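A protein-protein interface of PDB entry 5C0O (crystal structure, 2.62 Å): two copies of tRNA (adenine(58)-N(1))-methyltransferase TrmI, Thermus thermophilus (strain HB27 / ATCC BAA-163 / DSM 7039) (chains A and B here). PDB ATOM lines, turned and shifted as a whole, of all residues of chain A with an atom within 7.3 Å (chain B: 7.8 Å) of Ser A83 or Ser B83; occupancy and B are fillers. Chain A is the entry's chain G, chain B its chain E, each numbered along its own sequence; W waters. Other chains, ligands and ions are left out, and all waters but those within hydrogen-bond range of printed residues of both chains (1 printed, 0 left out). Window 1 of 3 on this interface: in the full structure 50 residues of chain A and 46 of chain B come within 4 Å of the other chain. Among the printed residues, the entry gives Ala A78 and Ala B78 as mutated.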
ATOM      1  N   THR A  77      -9.369 -20.350  21.606  1.00  0.00           N
ATOM      2  CA  THR A  77      -9.818 -20.030  20.262  1.00  0.00           C
ATOM      3  C   THR A  77      -8.591 -19.860  19.375  1.00  0.00           C
ATOM      4  O   THR A  77      -7.629 -19.195  19.760  1.00  0.00           O
ATOM      5  CB  THR A  77     -10.674 -18.746  20.255  1.00  0.00           C
ATOM      6  OG1 THR A  77     -11.882 -18.979  20.989  1.00  0.00           O
ATOM      7  CG2 THR A  77     -11.017 -18.301  18.832  1.00  0.00           C
ATOM      8  N   ALA A  78      -8.615 -20.471  18.198  1.00  0.00           N
ATOM      9  CA  ALA A  78      -7.483 -20.375  17.285  1.00  0.00           C
ATOM     10  C   ALA A  78      -7.316 -18.933  16.801  1.00  0.00           C
ATOM     11  O   ALA A  78      -8.307 -18.265  16.498  1.00  0.00           O
ATOM     12  CB  ALA A  78      -7.665 -21.319  16.111  1.00  0.00           C
ATOM     13  N   PRO A  79      -6.063 -18.448  16.726  1.00  0.00           N
ATOM     14  CA  PRO A  79      -5.800 -17.042  16.384  1.00  0.00           C
ATOM     15  C   PRO A  79      -6.388 -16.595  15.045  1.00  0.00           C
ATOM     16  O   PRO A  79      -6.672 -15.412  14.892  1.00  0.00           O
ATOM     17  CB  PRO A  79      -4.264 -16.963  16.350  1.00  0.00           C
ATOM     18  CG  PRO A  79      -3.776 -18.369  16.340  1.00  0.00           C
ATOM     19  CD  PRO A  79      -4.821 -19.183  17.014  1.00  0.00           C
ATOM     20  N   LYS A  80      -6.565 -17.510  14.097  1.00  0.00           N
ATOM     21  CA  LYS A  80      -7.175 -17.157  12.820  1.00  0.00           C
ATOM     22  C   LYS A  80      -8.662 -16.880  13.017  1.00  0.00           C
ATOM     23  O   LYS A  80      -9.231 -15.991  12.380  1.00  0.00           O
ATOM     24  CB  LYS A  80      -6.975 -18.270  11.788  1.00  0.00           C
ATOM     25  CG  LYS A  80      -7.625 -19.587  12.164  1.00  0.00           C
ATOM     26  CD  LYS A  80      -7.530 -20.601  11.049  1.00  0.00           C
ATOM     27  CE  LYS A  80      -8.352 -21.837  11.372  1.00  0.00           C
ATOM     28  NZ  LYS A  80      -9.814 -21.583  11.214  1.00  0.00           N
ATOM     29  N   ASP A  81      -9.282 -17.655  13.902  1.00  0.00           N
ATOM     30  CA  ASP A  81     -10.691 -17.478  14.228  1.00  0.00           C
ATOM     31  C   ASP A  81     -10.860 -16.307  15.191  1.00  0.00           C
ATOM     32  O   ASP A  81     -11.783 -15.505  15.055  1.00  0.00           O
ATOM     33  CB  ASP A  81     -11.266 -18.759  14.839  1.00  0.00           C
ATOM     34  CG  ASP A  81     -11.112 -19.962  13.929  1.00  0.00           C
ATOM     35  OD1 ASP A  81     -11.090 -19.777  12.694  1.00  0.00           O
ATOM     36  OD2 ASP A  81     -11.012 -21.094  14.448  1.00  0.00           O
ATOM     37  N   ALA A  82      -9.955 -16.218  16.161  1.00  0.00           N
ATOM     38  CA  ALA A  82      -9.964 -15.125  17.126  1.00  0.00           C
ATOM     39  C   ALA A  82      -9.741 -13.798  16.418  1.00  0.00           C
ATOM     40  O   ALA A  82     -10.371 -12.792  16.746  1.00  0.00           O
ATOM     41  CB  ALA A  82      -8.900 -15.346  18.186  1.00  0.00           C
ATOM     42  N   SER A  83      -8.834 -13.805  15.445  1.00  0.00           N
ATOM     43  CA  SER A  83      -8.598 -12.635  14.608  1.00  0.00           C
ATOM     44  C   SER A  83      -9.855 -12.257  13.831  1.00  0.00           C
ATOM     45  O   SER A  83     -10.237 -11.088  13.776  1.00  0.00           O
ATOM     46  CB  SER A  83      -7.449 -12.897  13.634  1.00  0.00           C
ATOM     47  OG  SER A  83      -7.277 -11.811  12.741  1.00  0.00           O
ATOM     48  N   ALA A  84     -10.497 -13.255  13.232  1.00  0.00           N
ATOM     49  CA  ALA A  84     -11.683 -13.021  12.420  1.00  0.00           C
ATOM     50  C   ALA A  84     -12.888 -12.669  13.288  1.00  0.00           C
ATOM     51  O   ALA A  84     -13.795 -11.968  12.839  1.00  0.00           O
ATOM     52  CB  ALA A  84     -11.986 -14.242  11.561  1.00  0.00           C
ATOM     53  N   MET A  85     -12.892 -13.153  14.527  1.00  0.00           N
ATOM     54  CA  MET A  85     -13.995 -12.879  15.442  1.00  0.00           C
ATOM     55  C   MET A  85     -14.083 -11.387  15.753  1.00  0.00           C
ATOM     56  O   MET A  85     -15.177 -10.838  15.885  1.00  0.00           O
ATOM     57  CB  MET A  85     -13.838 -13.684  16.735  1.00  0.00           C
ATOM     58  CG  MET A  85     -14.493 -15.061  16.686  1.00  0.00           C
ATOM     59  SD  MET A  85     -14.198 -16.066  18.159  1.00  0.00           S
ATOM     60  CE  MET A  85     -15.735 -15.863  19.054  1.00  0.00           C
ATOM     61  N   VAL A  86     -12.926 -10.739  15.853  1.00  0.00           N
ATOM     62  CA  VAL A  86     -12.845  -9.306  16.135  1.00  0.00           C
ATOM     63  C   VAL A  86     -13.485  -8.486  15.014  1.00  0.00           C
ATOM     64  O   VAL A  86     -14.241  -7.548  15.272  1.00  0.00           O
ATOM     65  CB  VAL A  86     -11.361  -8.870  16.330  1.00  0.00           C
ATOM     66  CG1 VAL A  86     -11.186  -7.331  16.296  1.00  0.00           C
ATOM     67  CG2 VAL A  86     -10.807  -9.454  17.623  1.00  0.00           C
ATOM     68  N   THR A  87     -13.177  -8.838  13.773  1.00  0.00           N
ATOM     69  CA  THR A  87     -13.650  -8.070  12.628  1.00  0.00           C
ATOM     70  C   THR A  87     -15.156  -8.251  12.444  1.00  0.00           C
ATOM     71  O   THR A  87     -15.859  -7.307  12.080  1.00  0.00           O
ATOM     72  CB  THR A  87     -12.890  -8.470  11.340  1.00  0.00           C
ATOM     73  OG1 THR A  87     -11.556  -7.949  11.398  1.00  0.00           O
ATOM     74  CG2 THR A  87     -13.574  -7.927  10.093  1.00  0.00           C
ATOM     75  N   LEU A  88     -15.653  -9.457  12.705  1.00  0.00           N
ATOM     76  CA  LEU A  88     -17.088  -9.716  12.623  1.00  0.00           C
ATOM     77  C   LEU A  88     -17.821  -8.958  13.721  1.00  0.00           C
ATOM     78  O   LEU A  88     -18.905  -8.417  13.501  1.00  0.00           O
ATOM     79  CB  LEU A  88     -17.384 -11.211  12.735  1.00  0.00           C
ATOM     80  CG  LEU A  88     -17.193 -12.037  11.463  1.00  0.00           C
ATOM     81  CD1 LEU A  88     -17.258 -13.518  11.785  1.00  0.00           C
ATOM     82  CD2 LEU A  88     -18.239 -11.675  10.414  1.00  0.00           C
ATOM     83  N   LEU A 107      -8.692 -15.839  23.358  1.00  0.00           N
ATOM     84  CA  LEU A 107      -9.521 -14.869  22.643  1.00  0.00           C
ATOM     85  C   LEU A 107      -9.701 -13.589  23.454  1.00  0.00           C
ATOM     86  O   LEU A 107      -9.926 -12.516  22.898  1.00  0.00           O
ATOM     87  CB  LEU A 107     -10.883 -15.489  22.317  1.00  0.00           C
ATOM     88  CG  LEU A 107     -12.043 -14.577  21.909  1.00  0.00           C
ATOM     89  CD1 LEU A 107     -11.779 -13.890  20.577  1.00  0.00           C
ATOM     90  CD2 LEU A 107     -13.316 -15.394  21.845  1.00  0.00           C
ATOM     91  N   PHE A 110      -7.093 -11.066  22.371  1.00  0.00           N
ATOM     92  CA  PHE A 110      -7.414 -10.512  21.060  1.00  0.00           C
ATOM     93  C   PHE A 110      -8.461  -9.411  21.187  1.00  0.00           C
ATOM     94  O   PHE A 110      -8.388  -8.387  20.508  1.00  0.00           O
ATOM     95  CB  PHE A 110      -7.921 -11.607  20.117  1.00  0.00           C
ATOM     96  CG  PHE A 110      -6.851 -12.204  19.245  1.00  0.00           C
ATOM     97  CD1 PHE A 110      -6.020 -13.198  19.728  1.00  0.00           C
ATOM     98  CD2 PHE A 110      -6.684 -11.774  17.940  1.00  0.00           C
ATOM     99  CE1 PHE A 110      -5.039 -13.749  18.926  1.00  0.00           C
ATOM    100  CE2 PHE A 110      -5.703 -12.322  17.135  1.00  0.00           C
ATOM    101  CZ  PHE A 110      -4.881 -13.311  17.630  1.00  0.00           C
ATOM    102  N   VAL A 221     -13.008 -20.137   8.558  1.00  0.00           N
ATOM    103  CA  VAL A 221     -11.755 -19.434   8.334  1.00  0.00           C
ATOM    104  C   VAL A 221     -10.655 -20.451   8.071  1.00  0.00           C
ATOM    105  O   VAL A 221     -10.569 -21.474   8.751  1.00  0.00           O
ATOM    106  CB  VAL A 221     -11.368 -18.556   9.531  1.00  0.00           C
ATOM    107  CG1 VAL A 221     -10.062 -17.816   9.253  1.00  0.00           C
ATOM    108  CG2 VAL A 221     -12.488 -17.578   9.852  1.00  0.00           C
ATOM    109  N   TRP A 223      -6.433 -20.338   7.356  1.00  0.00           N
ATOM    110  CA  TRP A 223      -5.113 -19.777   7.101  1.00  0.00           C
ATOM    111  C   TRP A 223      -4.240 -20.883   6.534  1.00  0.00           C
ATOM    112  O   TRP A 223      -3.696 -21.702   7.273  1.00  0.00           O
ATOM    113  CB  TRP A 223      -4.495 -19.195   8.372  1.00  0.00           C
ATOM    114  CG  TRP A 223      -5.047 -17.857   8.763  1.00  0.00           C
ATOM    115  CD1 TRP A 223      -6.136 -17.227   8.232  1.00  0.00           C
ATOM    116  CD2 TRP A 223      -4.525 -16.977   9.765  1.00  0.00           C
ATOM    117  NE1 TRP A 223      -6.325 -16.010   8.846  1.00  0.00           N
ATOM    118  CE2 TRP A 223      -5.349 -15.834   9.791  1.00  0.00           C
ATOM    119  CE3 TRP A 223      -3.441 -17.047  10.645  1.00  0.00           C
ATOM    120  CZ2 TRP A 223      -5.123 -14.771  10.664  1.00  0.00           C
ATOM    121  CZ3 TRP A 223      -3.218 -15.989  11.509  1.00  0.00           C
ATOM    122  CH2 TRP A 223      -4.055 -14.867  11.512  1.00  0.00           C
ATOM    123  N   LEU A 246     -17.832 -19.965  12.619  1.00  0.00           N
ATOM    124  CA  LEU A 246     -18.106 -18.674  13.241  1.00  0.00           C
ATOM    125  C   LEU A 246     -19.520 -18.227  12.887  1.00  0.00           C
ATOM    126  O   LEU A 246     -19.873 -18.141  11.710  1.00  0.00           O
ATOM    127  CB  LEU A 246     -17.084 -17.621  12.800  1.00  0.00           C
ATOM    128  CG  LEU A 246     -15.611 -17.909  13.111  1.00  0.00           C
ATOM    129  CD1 LEU A 246     -14.717 -16.853  12.476  1.00  0.00           C
ATOM    130  CD2 LEU A 246     -15.369 -17.984  14.613  1.00  0.00           C
ATOM    131  N   LEU B  67     -15.598  -0.937   3.697  1.00  0.00           N
ATOM    132  CA  LEU B  67     -14.610  -1.228   2.659  1.00  0.00           C
ATOM    133  C   LEU B  67     -15.240  -1.784   1.385  1.00  0.00           C
ATOM    134  O   LEU B  67     -14.838  -1.432   0.276  1.00  0.00           O
ATOM    135  CB  LEU B  67     -13.570  -2.223   3.182  1.00  0.00           C
ATOM    136  CG  LEU B  67     -12.195  -1.653   3.543  1.00  0.00           C
ATOM    137  CD1 LEU B  67     -12.270  -0.773   4.782  1.00  0.00           C
ATOM    138  CD2 LEU B  67     -11.196  -2.779   3.736  1.00  0.00           C
ATOM    139  N   THR B  77      -7.888  -3.162  -0.009  1.00  0.00           N
ATOM    140  CA  THR B  77      -7.502  -4.482   0.472  1.00  0.00           C
ATOM    141  C   THR B  77      -8.731  -5.204   1.019  1.00  0.00           C
ATOM    142  O   THR B  77      -9.568  -4.591   1.676  1.00  0.00           O
ATOM    143  CB  THR B  77      -6.422  -4.371   1.568  1.00  0.00           C
ATOM    144  OG1 THR B  77      -5.421  -3.426   1.160  1.00  0.00           O
ATOM    145  CG2 THR B  77      -5.776  -5.723   1.841  1.00  0.00           C
ATOM    146  N   ALA B  78      -8.847  -6.500   0.748  1.00  0.00           N
ATOM    147  CA  ALA B  78     -10.032  -7.247   1.162  1.00  0.00           C
ATOM    148  C   ALA B  78     -10.094  -7.365   2.686  1.00  0.00           C
ATOM    149  O   ALA B  78      -9.057  -7.525   3.333  1.00  0.00           O
ATOM    150  CB  ALA B  78     -10.045  -8.617   0.527  1.00  0.00           C
ATOM    151  N   PRO B  79     -11.308  -7.286   3.267  1.00  0.00           N
ATOM    152  CA  PRO B  79     -11.443  -7.321   4.728  1.00  0.00           C
ATOM    153  C   PRO B  79     -10.841  -8.562   5.385  1.00  0.00           C
ATOM    154  O   PRO B  79     -10.278  -8.457   6.475  1.00  0.00           O
ATOM    155  CB  PRO B  79     -12.961  -7.288   4.938  1.00  0.00           C
ATOM    156  CG  PRO B  79     -13.490  -6.614   3.728  1.00  0.00           C
ATOM    157  CD  PRO B  79     -12.613  -7.077   2.610  1.00  0.00           C
ATOM    158  N   LYS B  80     -10.957  -9.717   4.738  1.00  0.00           N
ATOM    159  CA  LYS B  80     -10.438 -10.952   5.313  1.00  0.00           C
ATOM    160  C   LYS B  80      -8.916 -10.902   5.407  1.00  0.00           C
ATOM    161  O   LYS B  80      -8.324 -11.430   6.352  1.00  0.00           O
ATOM    162  CB  LYS B  80     -10.879 -12.166   4.486  1.00  0.00           C
ATOM    163  CG  LYS B  80     -10.345 -12.192   3.065  1.00  0.00           C
ATOM    164  CD  LYS B  80     -10.772 -13.463   2.336  1.00  0.00           C
ATOM    165  CE  LYS B  80      -9.854 -13.774   1.159  1.00  0.00           C
ATOM    166  NZ  LYS B  80      -8.445 -14.017   1.585  1.00  0.00           N
ATOM    167  N   ASP B  81      -8.292 -10.255   4.429  1.00  0.00           N
ATOM    168  CA  ASP B  81      -6.838 -10.174   4.366  1.00  0.00           C
ATOM    169  C   ASP B  81      -6.321  -9.081   5.289  1.00  0.00           C
ATOM    170  O   ASP B  81      -5.362  -9.288   6.029  1.00  0.00           O
ATOM    171  CB  ASP B  81      -6.381  -9.918   2.931  1.00  0.00           C
ATOM    172  CG  ASP B  81      -6.833 -11.004   1.977  1.00  0.00           C
ATOM    173  OD1 ASP B  81      -6.707 -12.195   2.330  1.00  0.00           O
ATOM    174  OD2 ASP B  81      -7.319 -10.670   0.876  1.00  0.00           O
ATOM    175  N   ALA B  82      -6.964  -7.917   5.240  1.00  0.00           N
ATOM    176  CA  ALA B  82      -6.596  -6.799   6.101  1.00  0.00           C
ATOM    177  C   ALA B  82      -6.690  -7.213   7.565  1.00  0.00           C
ATOM    178  O   ALA B  82      -5.845  -6.845   8.383  1.00  0.00           O
ATOM    179  CB  ALA B  82      -7.492  -5.603   5.828  1.00  0.00           C
ATOM    180  N   SER B  83      -7.727  -7.979   7.882  1.00  0.00           N
ATOM    181  CA  SER B  83      -7.925  -8.503   9.226  1.00  0.00           C
ATOM    182  C   SER B  83      -6.732  -9.345   9.653  1.00  0.00           C
ATOM    183  O   SER B  83      -6.214  -9.190  10.759  1.00  0.00           O
ATOM    184  CB  SER B  83      -9.208  -9.339   9.291  1.00  0.00           C
ATOM    185  OG  SER B  83      -9.497  -9.741  10.619  1.00  0.00           O
ATOM    186  N   ALA B  84      -6.299 -10.232   8.762  1.00  0.00           N
ATOM    187  CA  ALA B  84      -5.211 -11.156   9.061  1.00  0.00           C
ATOM    188  C   ALA B  84      -3.866 -10.442   9.115  1.00  0.00           C
ATOM    189  O   ALA B  84      -2.980 -10.838   9.871  1.00  0.00           O
ATOM    190  CB  ALA B  84      -5.175 -12.278   8.028  1.00  0.00           C
ATOM    191  N   MET B  85      -3.719  -9.389   8.317  1.00  0.00           N
ATOM    192  CA  MET B  85      -2.463  -8.649   8.244  1.00  0.00           C
ATOM    193  C   MET B  85      -2.147  -7.962   9.569  1.00  0.00           C
ATOM    194  O   MET B  85      -0.992  -7.897   9.986  1.00  0.00           O
ATOM    195  CB  MET B  85      -2.514  -7.608   7.122  1.00  0.00           C
ATOM    196  CG  MET B  85      -2.322  -8.183   5.730  1.00  0.00           C
ATOM    197  SD  MET B  85      -2.446  -6.929   4.445  1.00  0.00           S
ATOM    198  CE  MET B  85      -0.724  -6.539   4.167  1.00  0.00           C
ATOM    199  N   VAL B  86      -3.181  -7.449  10.222  1.00  0.00           N
ATOM    200  CA  VAL B  86      -3.031  -6.785  11.511  1.00  0.00           C
ATOM    201  C   VAL B  86      -2.543  -7.785  12.562  1.00  0.00           C
ATOM    202  O   VAL B  86      -1.767  -7.436  13.453  1.00  0.00           O
ATOM    203  CB  VAL B  86      -4.382  -6.119  11.926  1.00  0.00           C
ATOM    204  CG1 VAL B  86      -4.613  -6.080  13.469  1.00  0.00           C
ATOM    205  CG2 VAL B  86      -4.492  -4.715  11.303  1.00  0.00           C
ATOM    206  N   THR B  87      -2.995  -9.028  12.449  1.00  0.00           N
ATOM    207  CA  THR B  87      -2.595 -10.068  13.388  1.00  0.00           C
ATOM    208  C   THR B  87      -1.161 -10.520  13.125  1.00  0.00           C
ATOM    209  O   THR B  87      -0.414 -10.820  14.058  1.00  0.00           O
ATOM    210  CB  THR B  87      -3.553 -11.275  13.311  1.00  0.00           C
ATOM    211  OG1 THR B  87      -4.837 -10.883  13.806  1.00  0.00           O
ATOM    212  CG2 THR B  87      -3.037 -12.467  14.130  1.00  0.00           C
ATOM    213  N   LEU B  88      -0.777 -10.559  11.854  1.00  0.00           N
ATOM    214  CA  LEU B  88       0.568 -10.976  11.472  1.00  0.00           C
ATOM    215  C   LEU B  88       1.591  -9.903  11.828  1.00  0.00           C
ATOM    216  O   LEU B  88       2.746 -10.210  12.129  1.00  0.00           O
ATOM    217  CB  LEU B  88       0.624 -11.288   9.977  1.00  0.00           C
ATOM    218  CG  LEU B  88      -0.134 -12.554   9.575  1.00  0.00           C
ATOM    219  CD1 LEU B  88      -0.426 -12.567   8.080  1.00  0.00           C
ATOM    220  CD2 LEU B  88       0.659 -13.788   9.982  1.00  0.00           C
ATOM    221  N   LEU B  89       1.159  -8.648  11.793  1.00  0.00           N
ATOM    222  CA  LEU B  89       2.009  -7.533  12.188  1.00  0.00           C
ATOM    223  C   LEU B  89       2.080  -7.410  13.711  1.00  0.00           C
ATOM    224  O   LEU B  89       2.891  -6.648  14.238  1.00  0.00           O
ATOM    225  CB  LEU B  89       1.494  -6.229  11.571  1.00  0.00           C
ATOM    226  CG  LEU B  89       1.657  -6.115  10.054  1.00  0.00           C
ATOM    227  CD1 LEU B  89       0.896  -4.927   9.497  1.00  0.00           C
ATOM    228  CD2 LEU B  89       3.132  -6.016   9.689  1.00  0.00           C
ATOM    229  N   LEU B 107      -7.033  -0.680   4.103  1.00  0.00           N
ATOM    230  CA  LEU B 107      -6.111  -1.291   5.055  1.00  0.00           C
ATOM    231  C   LEU B 107      -5.727  -0.283   6.133  1.00  0.00           C
ATOM    232  O   LEU B 107      -5.456  -0.650   7.275  1.00  0.00           O
ATOM    233  CB  LEU B 107      -4.867  -1.806   4.328  1.00  0.00           C
ATOM    234  CG  LEU B 107      -3.775  -2.508   5.139  1.00  0.00           C
ATOM    235  CD1 LEU B 107      -4.318  -3.726   5.875  1.00  0.00           C
ATOM    236  CD2 LEU B 107      -2.644  -2.904   4.198  1.00  0.00           C
ATOM    237  N   PHE B 110      -8.150  -0.423   9.138  1.00  0.00           N
ATOM    238  CA  PHE B 110      -7.837  -1.573   9.978  1.00  0.00           C
ATOM    239  C   PHE B 110      -6.619  -1.272  10.841  1.00  0.00           C
ATOM    240  O   PHE B 110      -6.599  -1.576  12.033  1.00  0.00           O
ATOM    241  CB  PHE B 110      -7.584  -2.818   9.125  1.00  0.00           C
ATOM    242  CG  PHE B 110      -8.841  -3.514   8.682  1.00  0.00           C
ATOM    243  CD1 PHE B 110      -9.571  -3.036   7.606  1.00  0.00           C
ATOM    244  CD2 PHE B 110      -9.291  -4.646   9.340  1.00  0.00           C
ATOM    245  CE1 PHE B 110     -10.724  -3.674   7.198  1.00  0.00           C
ATOM    246  CE2 PHE B 110     -10.447  -5.287   8.936  1.00  0.00           C
ATOM    247  CZ  PHE B 110     -11.163  -4.800   7.862  1.00  0.00           C
ATOM    248  N   VAL B 221      -5.512 -16.723   2.915  1.00  0.00           N
ATOM    249  CA  VAL B 221      -6.636 -16.553   3.825  1.00  0.00           C
ATOM    250  C   VAL B 221      -7.927 -16.887   3.091  1.00  0.00           C
ATOM    251  O   VAL B 221      -8.108 -16.505   1.933  1.00  0.00           O
ATOM    252  CB  VAL B 221      -6.702 -15.122   4.384  1.00  0.00           C
ATOM    253  CG1 VAL B 221      -7.904 -14.961   5.299  1.00  0.00           C
ATOM    254  CG2 VAL B 221      -5.422 -14.789   5.132  1.00  0.00           C
ATOM    255  N   TRP B 223     -12.162 -16.955   3.882  1.00  0.00           N
ATOM    256  CA  TRP B 223     -13.408 -16.839   4.626  1.00  0.00           C
ATOM    257  C   TRP B 223     -14.515 -17.491   3.812  1.00  0.00           C
ATOM    258  O   TRP B 223     -15.106 -16.874   2.922  1.00  0.00           O
ATOM    259  CB  TRP B 223     -13.738 -15.377   4.927  1.00  0.00           C
ATOM    260  CG  TRP B 223     -12.881 -14.784   6.006  1.00  0.00           C
ATOM    261  CD1 TRP B 223     -11.763 -15.335   6.561  1.00  0.00           C
ATOM    262  CD2 TRP B 223     -13.081 -13.530   6.668  1.00  0.00           C
ATOM    263  NE1 TRP B 223     -11.251 -14.499   7.525  1.00  0.00           N
ATOM    264  CE2 TRP B 223     -12.042 -13.385   7.611  1.00  0.00           C
ATOM    265  CE3 TRP B 223     -14.035 -12.516   6.555  1.00  0.00           C
ATOM    266  CZ2 TRP B 223     -11.932 -12.268   8.432  1.00  0.00           C
ATOM    267  CZ3 TRP B 223     -13.923 -11.407   7.373  1.00  0.00           C
ATOM    268  CH2 TRP B 223     -12.880 -11.292   8.299  1.00  0.00           C
ATOM    269  N   LEU B 246      -0.469 -13.608   1.510  1.00  0.00           N
ATOM    270  CA  LEU B 246       0.164 -12.768   2.517  1.00  0.00           C
ATOM    271  C   LEU B 246       1.558 -13.300   2.810  1.00  0.00           C
ATOM    272  O   LEU B 246       1.721 -14.461   3.182  1.00  0.00           O
ATOM    273  CB  LEU B 246      -0.673 -12.723   3.799  1.00  0.00           C
ATOM    274  CG  LEU B 246      -2.079 -12.122   3.690  1.00  0.00           C
ATOM    275  CD1 LEU B 246      -2.707 -11.978   5.066  1.00  0.00           C
ATOM    276  CD2 LEU B 246      -2.053 -10.779   2.981  1.00  0.00           C
HETATM  277  O   HOH W   1      -8.100  -8.937  12.786  1.00  0.00           O
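Of the 17 printed residues of chain A, 6 touch a printed residue of chain B.
Hydrophobic or aromatic side chains of chain B within 4 Å of the printed part of chain A: Ala B84, Phe B110 and Trp B223.
Among the printed residues, no Asp or Glu carboxylate lies within 4 Å of a Lys or Arg side-chain nitrogen of the other chain.
Water W1 bridges OG of Ser B83 (2.7 Å) and OG of Ser A83 (3.0 Å).
NZ of Lys A80 lies within hydrogen-bond range of O of Val A221, at 2.6 Å.
Ser A83 touches its own counterpart, Ser B83.
Ser A83 touches Thr B87, and with the chains exchanged Thr A87 touches Ser B83.
Thr A87 touches Phe B110, and with the chains exchanged Phe A110 touches Thr B87.
Thr A87 touches Trp B223, and with the chains exchanged Trp A223 touches Thr B87.
Ala A84 touches Trp B223 (CB to CZ2, 3.7 Å).
Thr A87 touches Phe B110 (OG1 to CE2, 3.8 Å).
Thr A87 touches Trp B223 (CG2 to CH2, 3.9 Å).
Phe A110 touches Thr B87.
Trp B223 touches Val A221.
Trp A223 touches Ala B84.
Trp A223 touches Thr B87 (CH2 to CG2, 3.7 Å).
The side-chain hydroxyl of Ser A83 sits at hydrogen-bond distance from the backbone carbonyl oxygen of Ser B83 (3.5 Å).
OG of Ser B83 sits at hydrogen-bond distance from OG1 of Thr A87 (2.8 Å).
The side-chain hydroxyl of Thr B87 is in hydrogen-bond range of the side-chain hydroxyl of Ser A83, at 2.8 Å.
Ser A83 touches two residues of chain B.
Ser B83 touches two residues of chain A.
No residue of chain B comes within 4 Å of Ala A82.
Of the printed residues of chain B, Thr A87 touches Ser B83 (2.8 Å), Phe B110 (3.8 Å) and Trp B223 (3.9 Å).
Of the printed residues of chain A, Thr B87 touches Ser A83 (2.8 Å), Phe A110 (3.7 Å) and Trp A223 (3.7 Å).
Of the printed residues of chain A, Ala B84 touches Trp A223 (3.6 Å).
Of the printed residues of chain A, Phe B110 touches Thr A87.
The nearest residue of chain A that does not touch Ser B83 is Ala A84 (4.3 Å).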
